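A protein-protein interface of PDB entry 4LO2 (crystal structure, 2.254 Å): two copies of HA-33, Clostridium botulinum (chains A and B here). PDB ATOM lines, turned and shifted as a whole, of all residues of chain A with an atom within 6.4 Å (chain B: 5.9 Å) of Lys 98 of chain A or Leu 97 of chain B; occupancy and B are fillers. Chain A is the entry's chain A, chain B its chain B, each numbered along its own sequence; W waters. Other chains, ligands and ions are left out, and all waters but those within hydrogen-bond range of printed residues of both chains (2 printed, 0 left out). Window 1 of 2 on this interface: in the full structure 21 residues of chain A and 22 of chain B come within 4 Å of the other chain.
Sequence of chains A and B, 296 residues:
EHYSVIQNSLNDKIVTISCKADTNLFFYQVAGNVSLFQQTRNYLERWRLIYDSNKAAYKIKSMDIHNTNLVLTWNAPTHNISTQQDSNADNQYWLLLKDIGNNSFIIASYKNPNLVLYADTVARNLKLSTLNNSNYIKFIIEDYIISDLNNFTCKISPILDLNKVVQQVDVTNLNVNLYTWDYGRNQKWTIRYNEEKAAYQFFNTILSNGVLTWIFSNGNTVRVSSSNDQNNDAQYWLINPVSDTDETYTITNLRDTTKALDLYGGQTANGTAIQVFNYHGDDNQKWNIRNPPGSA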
ATOM      1  N   LEU A  96     -11.376  15.255 -24.507  1.00  0.00           N
ATOM      2  CA  LEU A  96     -11.885  13.927 -24.835  1.00  0.00           C
ATOM      3  C   LEU A  96     -13.158  13.736 -24.058  1.00  0.00           C
ATOM      4  O   LEU A  96     -13.128  13.565 -22.839  1.00  0.00           O
ATOM      5  CB  LEU A  96     -10.865  12.836 -24.470  1.00  0.00           C
ATOM      6  CG  LEU A  96      -9.533  13.020 -25.184  1.00  0.00           C
ATOM      7  CD1 LEU A  96      -8.596  11.849 -24.886  1.00  0.00           C
ATOM      8  CD2 LEU A  96      -9.756  13.180 -26.685  1.00  0.00           C
ATOM      9  N   LEU A  97     -14.280  13.817 -24.768  1.00  0.00           N
ATOM     10  CA  LEU A  97     -15.577  13.760 -24.134  1.00  0.00           C
ATOM     11  C   LEU A  97     -16.206  12.419 -24.451  1.00  0.00           C
ATOM     12  O   LEU A  97     -16.532  12.130 -25.596  1.00  0.00           O
ATOM     13  CB  LEU A  97     -16.460  14.904 -24.646  1.00  0.00           C
ATOM     14  CG  LEU A  97     -15.780  16.258 -24.505  1.00  0.00           C
ATOM     15  CD1 LEU A  97     -16.537  17.315 -25.298  1.00  0.00           C
ATOM     16  CD2 LEU A  97     -15.675  16.630 -23.025  1.00  0.00           C
ATOM     17  N   LYS A  98     -16.373  11.595 -23.433  1.00  0.00           N
ATOM     18  CA  LYS A  98     -16.890  10.255 -23.644  1.00  0.00           C
ATOM     19  C   LYS A  98     -18.410  10.264 -23.633  1.00  0.00           C
ATOM     20  O   LYS A  98     -19.038  10.664 -22.647  1.00  0.00           O
ATOM     21  CB  LYS A  98     -16.366   9.295 -22.566  1.00  0.00           C
ATOM     22  CG  LYS A  98     -16.411   7.826 -22.971  1.00  0.00           C
ATOM     23  CD  LYS A  98     -16.005   6.927 -21.796  1.00  0.00           C
ATOM     24  CE  LYS A  98     -15.876   5.473 -22.222  1.00  0.00           C
ATOM     25  NZ  LYS A  98     -15.624   4.596 -21.037  1.00  0.00           N
ATOM     26  N   ASP A  99     -18.996   9.817 -24.738  1.00  0.00           N
ATOM     27  CA  ASP A  99     -20.448   9.700 -24.839  1.00  0.00           C
ATOM     28  C   ASP A  99     -20.856   8.407 -24.154  1.00  0.00           C
ATOM     29  O   ASP A  99     -20.780   7.341 -24.746  1.00  0.00           O
ATOM     30  CB  ASP A  99     -20.869   9.673 -26.311  1.00  0.00           C
ATOM     31  CG  ASP A  99     -22.371   9.845 -26.502  1.00  0.00           C
ATOM     32  OD1 ASP A  99     -23.162   9.361 -25.661  1.00  0.00           O
ATOM     33  OD2 ASP A  99     -22.760  10.473 -27.508  1.00  0.00           O
ATOM     34  N   ILE A 100     -21.268   8.509 -22.897  1.00  0.00           N
ATOM     35  CA  ILE A 100     -21.584   7.333 -22.098  1.00  0.00           C
ATOM     36  C   ILE A 100     -22.776   6.576 -22.676  1.00  0.00           C
ATOM     37  O   ILE A 100     -23.754   7.172 -23.136  1.00  0.00           O
ATOM     38  CB  ILE A 100     -21.906   7.723 -20.647  1.00  0.00           C
ATOM     39  CG1 ILE A 100     -20.832   8.657 -20.108  1.00  0.00           C
ATOM     40  CG2 ILE A 100     -21.964   6.490 -19.772  1.00  0.00           C
ATOM     41  CD1 ILE A 100     -19.460   8.023 -20.045  1.00  0.00           C
ATOM     42  N   ASN A 103     -20.154   4.276 -25.891  1.00  0.00           N
ATOM     43  CA  ASN A 103     -18.764   3.828 -25.909  1.00  0.00           C
ATOM     44  C   ASN A 103     -17.937   4.504 -27.012  1.00  0.00           C
ATOM     45  O   ASN A 103     -17.197   3.852 -27.756  1.00  0.00           O
ATOM     46  CB  ASN A 103     -18.703   2.307 -26.034  1.00  0.00           C
ATOM     47  CG  ASN A 103     -17.413   1.724 -25.475  1.00  0.00           C
ATOM     48  OD1 ASN A 103     -16.729   2.359 -24.663  1.00  0.00           O
ATOM     49  ND2 ASN A 103     -17.076   0.508 -25.902  1.00  0.00           N
ATOM     50  N   SER A 104     -18.097   5.812 -27.136  1.00  0.00           N
ATOM     51  CA  SER A 104     -17.426   6.537 -28.186  1.00  0.00           C
ATOM     52  C   SER A 104     -17.075   7.924 -27.669  1.00  0.00           C
ATOM     53  O   SER A 104     -17.601   8.363 -26.646  1.00  0.00           O
ATOM     54  CB  SER A 104     -18.300   6.581 -29.443  1.00  0.00           C
ATOM     55  OG  SER A 104     -19.385   7.474 -29.307  1.00  0.00           O
ATOM     56  N   PHE A 105     -16.160   8.592 -28.352  1.00  0.00           N
ATOM     57  CA  PHE A 105     -15.687   9.897 -27.910  1.00  0.00           C
ATOM     58  C   PHE A 105     -16.005  10.959 -28.937  1.00  0.00           C
ATOM     59  O   PHE A 105     -15.887  10.727 -30.132  1.00  0.00           O
ATOM     60  CB  PHE A 105     -14.166   9.887 -27.722  1.00  0.00           C
ATOM     61  CG  PHE A 105     -13.705   9.160 -26.485  1.00  0.00           C
ATOM     62  CD1 PHE A 105     -13.345   9.870 -25.348  1.00  0.00           C
ATOM     63  CD2 PHE A 105     -13.629   7.781 -26.467  1.00  0.00           C
ATOM     64  CE1 PHE A 105     -12.916   9.215 -24.209  1.00  0.00           C
ATOM     65  CE2 PHE A 105     -13.188   7.103 -25.324  1.00  0.00           C
ATOM     66  CZ  PHE A 105     -12.835   7.818 -24.198  1.00  0.00           C
ATOM     67  N   ILE A 106     -16.420  12.124 -28.456  1.00  0.00           N
ATOM     68  CA  ILE A 106     -16.331  13.345 -29.234  1.00  0.00           C
ATOM     69  C   ILE A 106     -14.997  13.993 -28.859  1.00  0.00           C
ATOM     70  O   ILE A 106     -14.622  14.033 -27.687  1.00  0.00           O
ATOM     71  CB  ILE A 106     -17.509  14.276 -28.920  1.00  0.00           C
ATOM     72  CG1 ILE A 106     -18.803  13.625 -29.400  1.00  0.00           C
ATOM     73  CG2 ILE A 106     -17.302  15.656 -29.580  1.00  0.00           C
ATOM     74  CD1 ILE A 106     -20.065  14.426 -29.079  1.00  0.00           C
ATOM     75  N   LEU A 131     -21.110  20.666 -34.001  1.00  0.00           N
ATOM     76  CA  LEU A 131     -21.680  19.393 -33.557  1.00  0.00           C
ATOM     77  C   LEU A 131     -22.983  19.037 -34.236  1.00  0.00           C
ATOM     78  O   LEU A 131     -23.716  19.905 -34.713  1.00  0.00           O
ATOM     79  CB  LEU A 131     -21.903  19.391 -32.049  1.00  0.00           C
ATOM     80  CG  LEU A 131     -20.614  19.407 -31.234  1.00  0.00           C
ATOM     81  CD1 LEU A 131     -20.175  20.826 -30.950  1.00  0.00           C
ATOM     82  CD2 LEU A 131     -20.773  18.610 -29.963  1.00  0.00           C
ATOM     83  N   LEU B  95     -27.450  14.483 -24.247  1.00  0.00           N
ATOM     84  CA  LEU B  95     -26.237  13.693 -24.405  1.00  0.00           C
ATOM     85  C   LEU B  95     -25.413  13.931 -23.157  1.00  0.00           C
ATOM     86  O   LEU B  95     -25.188  15.079 -22.763  1.00  0.00           O
ATOM     87  CB  LEU B  95     -25.440  14.154 -25.616  1.00  0.00           C
ATOM     88  CG  LEU B  95     -26.192  14.283 -26.935  1.00  0.00           C
ATOM     89  CD1 LEU B  95     -25.213  14.672 -28.020  1.00  0.00           C
ATOM     90  CD2 LEU B  95     -26.830  12.966 -27.262  1.00  0.00           C
ATOM     91  N   LEU B  96     -24.990  12.851 -22.519  1.00  0.00           N
ATOM     92  CA  LEU B  96     -24.177  12.969 -21.320  1.00  0.00           C
ATOM     93  C   LEU B  96     -22.752  12.693 -21.741  1.00  0.00           C
ATOM     94  O   LEU B  96     -22.397  11.553 -22.042  1.00  0.00           O
ATOM     95  CB  LEU B  96     -24.647  11.977 -20.253  1.00  0.00           C
ATOM     96  CG  LEU B  96     -26.102  12.166 -19.777  1.00  0.00           C
ATOM     97  CD1 LEU B  96     -26.453  11.226 -18.623  1.00  0.00           C
ATOM     98  CD2 LEU B  96     -26.411  13.606 -19.400  1.00  0.00           C
ATOM     99  N   LEU B  97     -21.941  13.743 -21.800  1.00  0.00           N
ATOM    100  CA  LEU B  97     -20.572  13.598 -22.274  1.00  0.00           C
ATOM    101  C   LEU B  97     -19.633  13.729 -21.093  1.00  0.00           C
ATOM    102  O   LEU B  97     -19.557  14.786 -20.473  1.00  0.00           O
ATOM    103  CB  LEU B  97     -20.263  14.676 -23.312  1.00  0.00           C
ATOM    104  CG  LEU B  97     -21.308  14.747 -24.423  1.00  0.00           C
ATOM    105  CD1 LEU B  97     -21.098  15.982 -25.310  1.00  0.00           C
ATOM    106  CD2 LEU B  97     -21.271  13.458 -25.249  1.00  0.00           C
ATOM    107  N   LYS B  98     -18.922  12.660 -20.767  1.00  0.00           N
ATOM    108  CA  LYS B  98     -18.037  12.718 -19.629  1.00  0.00           C
ATOM    109  C   LYS B  98     -16.677  13.249 -20.060  1.00  0.00           C
ATOM    110  O   LYS B  98     -16.014  12.662 -20.913  1.00  0.00           O
ATOM    111  CB  LYS B  98     -17.887  11.339 -18.984  1.00  0.00           C
ATOM    112  CG  LYS B  98     -17.134  11.371 -17.667  1.00  0.00           C
ATOM    113  CD  LYS B  98     -17.323  10.087 -16.891  1.00  0.00           C
ATOM    114  CE  LYS B  98     -16.439  10.075 -15.657  1.00  0.00           C
ATOM    115  NZ  LYS B  98     -16.984   9.163 -14.612  1.00  0.00           N
ATOM    116  N   ASP B  99     -16.274  14.370 -19.469  1.00  0.00           N
ATOM    117  CA  ASP B  99     -14.947  14.927 -19.706  1.00  0.00           C
ATOM    118  C   ASP B  99     -13.904  14.124 -18.925  1.00  0.00           C
ATOM    119  O   ASP B  99     -13.732  14.330 -17.728  1.00  0.00           O
ATOM    120  CB  ASP B  99     -14.920  16.398 -19.276  1.00  0.00           C
ATOM    121  CG  ASP B  99     -13.672  17.127 -19.741  1.00  0.00           C
ATOM    122  OD1 ASP B  99     -12.672  16.472 -20.111  1.00  0.00           O
ATOM    123  OD2 ASP B  99     -13.692  18.371 -19.724  1.00  0.00           O
ATOM    124  N   ILE B 100     -13.199  13.222 -19.607  1.00  0.00           N
ATOM    125  CA  ILE B 100     -12.216  12.371 -18.944  1.00  0.00           C
ATOM    126  C   ILE B 100     -11.032  13.180 -18.404  1.00  0.00           C
ATOM    127  O   ILE B 100     -10.560  14.124 -19.035  1.00  0.00           O
ATOM    128  CB  ILE B 100     -11.713  11.258 -19.873  1.00  0.00           C
ATOM    129  CG1 ILE B 100     -12.895  10.603 -20.573  1.00  0.00           C
ATOM    130  CG2 ILE B 100     -10.947  10.211 -19.083  1.00  0.00           C
ATOM    131  CD1 ILE B 100     -13.848   9.920 -19.628  1.00  0.00           C
ATOM    132  N   SER B 104     -16.070  15.212 -14.794  1.00  0.00           N
ATOM    133  CA  SER B 104     -17.288  16.001 -14.816  1.00  0.00           C
ATOM    134  C   SER B 104     -17.979  15.764 -16.143  1.00  0.00           C
ATOM    135  O   SER B 104     -17.392  15.177 -17.067  1.00  0.00           O
ATOM    136  CB  SER B 104     -16.972  17.483 -14.614  1.00  0.00           C
ATOM    137  OG  SER B 104     -16.243  17.994 -15.729  1.00  0.00           O
ATOM    138  N   PHE B 105     -19.226  16.205 -16.230  1.00  0.00           N
ATOM    139  CA  PHE B 105     -20.061  15.942 -17.390  1.00  0.00           C
ATOM    140  C   PHE B 105     -20.475  17.233 -18.070  1.00  0.00           C
ATOM    141  O   PHE B 105     -20.790  18.222 -17.418  1.00  0.00           O
ATOM    142  CB  PHE B 105     -21.346  15.232 -16.968  1.00  0.00           C
ATOM    143  CG  PHE B 105     -21.195  13.755 -16.754  1.00  0.00           C
ATOM    144  CD1 PHE B 105     -21.459  12.869 -17.784  1.00  0.00           C
ATOM    145  CD2 PHE B 105     -20.824  13.255 -15.512  1.00  0.00           C
ATOM    146  CE1 PHE B 105     -21.335  11.502 -17.594  1.00  0.00           C
ATOM    147  CE2 PHE B 105     -20.692  11.893 -15.310  1.00  0.00           C
ATOM    148  CZ  PHE B 105     -20.951  11.013 -16.345  1.00  0.00           C
ATOM    149  N   ILE B 106     -20.494  17.206 -19.393  1.00  0.00           N
ATOM    150  CA  ILE B 106     -21.175  18.210 -20.170  1.00  0.00           C
ATOM    151  C   ILE B 106     -22.537  17.638 -20.559  1.00  0.00           C
ATOM    152  O   ILE B 106     -22.653  16.460 -20.924  1.00  0.00           O
ATOM    153  CB  ILE B 106     -20.343  18.574 -21.404  1.00  0.00           C
ATOM    154  CG1 ILE B 106     -19.115  19.379 -20.962  1.00  0.00           C
ATOM    155  CG2 ILE B 106     -21.179  19.350 -22.393  1.00  0.00           C
ATOM    156  CD1 ILE B 106     -18.046  19.493 -22.027  1.00  0.00           C
ATOM    157  N   ILE B 107     -23.584  18.441 -20.429  1.00  0.00           N
ATOM    158  CA  ILE B 107     -24.922  17.944 -20.729  1.00  0.00           C
ATOM    159  C   ILE B 107     -25.497  18.686 -21.936  1.00  0.00           C
ATOM    160  O   ILE B 107     -25.935  19.828 -21.812  1.00  0.00           O
ATOM    161  CB  ILE B 107     -25.834  18.095 -19.507  1.00  0.00           C
ATOM    162  CG1 ILE B 107     -25.228  17.346 -18.308  1.00  0.00           C
ATOM    163  CG2 ILE B 107     -27.237  17.591 -19.817  1.00  0.00           C
ATOM    164  CD1 ILE B 107     -25.958  17.627 -16.980  1.00  0.00           C
ATOM    165  N   ALA B 108     -25.482  18.030 -23.098  1.00  0.00           N
ATOM    166  CA  ALA B 108     -25.789  18.684 -24.369  1.00  0.00           C
ATOM    167  C   ALA B 108     -27.197  18.353 -24.850  1.00  0.00           C
ATOM    168  O   ALA B 108     -27.654  17.233 -24.697  1.00  0.00           O
ATOM    169  CB  ALA B 108     -24.735  18.280 -25.459  1.00  0.00           C
HETATM  170  O   HOH W   1     -25.266  10.475 -24.278  1.00  0.00           O
HETATM  171  O   HOH W   2     -10.641  16.243 -21.742  1.00  0.00           O
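Water W2 lies within hydrogen-bond range of the side-chain carboxylate of Asp 99 of chain B, the backbone NH of Leu 96 of chain A and the backbone carbonyl oxygen of Ile 100 of chain B. Water W1 lies within hydrogen-bond range of OD1 of Asp 99 of chain A (2.8 Å) and N of Leu 96 of chain B (3.0 Å).
Among the printed residues, merely in contact across the chains: Lys 98 of chain A with Leu 97 of chain B, Leu 97 of chain A with Lys 98 of chain B, Lys 98 of chain A with Leu 96 of chain B, Leu 96 of chain A with Lys 98 of chain B, Leu 97 of chain A with Asp 99 of chain B, Ile 100 of chain A with Lys 98 of chain B, Ile 100 of chain A with Phe 105 of chain B, Leu 97 of chain A with Ile 106 of chain B, Asp 99 of chain A with Leu 97 of chain B, Leu 96 of chain A with Asp 99 of chain B, Asp 99 of chain A with Leu 96 of chain B, Phe 105 of chain A with Ile 100 of chain B and Lys 98 of chain A with Ile 100 of chain B.
Of the 10 printed residues of chain A, 6 touch a printed residue of chain B. Printed residues of chain A that touch a printed residue of chain B: Leu 96, Leu 97, Lys 98, Asp 99, Ile 100 and Phe 105. Of the 11 printed residues of chain B, 7 touch a printed residue of chain A. Hydrophobic or aromatic side chains of chain B within 4 Å of the printed part of chain A: Leu 97, Ile 100, Phe 105 and Ile 106. Among the printed residues, 16 pairs touch across the chains.
The backbone NH (N) of Asp 99 of chain B lies within hydrogen-bond range of the backbone carbonyl oxygen (O) of Ser 104 of chain B. The backbone carbonyl oxygen of Leu 97 of chain A is in hydrogen-bond range of the backbone NH of Ile 106 of chain A (2.9 Å). The backbone NH (N) of Asp 99 of chain A sits at hydrogen-bond distance from the backbone carbonyl oxygen (O) of Ser 104 of chain A (2.8 Å). O of Leu 97 of chain B is in hydrogen-bond range of N of Ile 106 of chain B (2.8 Å).
Leu 97 of chain A touches Lys 98 of chain B, and with the chains exchanged Lys 98 of chain A touches Leu 97 of chain B. Leu 97 of chain A touches Ile 106 of chain B, but with the chains exchanged Ile 106 of chain A does not touch Leu 97 of chain B (4.1 Å). Lys 98 of chain A touches its own counterpart, Lys 98 of chain B. Lys 98 of chain A touches Ile 100 of chain B, and with the chains exchanged Ile 100 of chain A touches Lys 98 of chain B. Of the 16 pairs that touch across the chains among the printed residues, 15 have their exchanged pair printed and touching as well.
N of Ile 100 of chain A lies within hydrogen-bond range of O of Leu 96 of chain B, at 3.4 Å. O of Leu 96 of chain A sits at hydrogen-bond distance from N of Ile 100 of chain B (3.3 Å). The backbone carbonyl oxygen (O) of Lys 98 of chain A sits at hydrogen-bond distance from the backbone NH (N) of Lys 98 of chain B, 2.7 Å away.
Lys 98 of chain A touches just these residues of chain B: Leu 96, Leu 97, Lys 98 and Ile 100. Printed residues of chain B within 4 Å of Ile 100 of chain A: Leu 96, Lys 98 and Phe 105. Of the printed residues of chain B, Phe 105 of chain A touches Ile 100. Of the printed residues of chain A, Leu 96 of chain B touches Lys 98 (3.5 Å), Asp 99 (3.9 Å) and Ile 100 (3.4 Å). Leu 97 of chain B touches just these residues of chain A: Lys 98 (3.3 Å) and Asp 99 (3.9 Å). Of the printed residues of chain A, Lys 98 of chain B touches Leu 96 (3.6 Å), Leu 97 (3.4 Å), Lys 98 (2.7 Å) and Ile 100 (3.8 Å). Of the printed residues of chain A, Phe 105 of chain B touches Ile 100.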
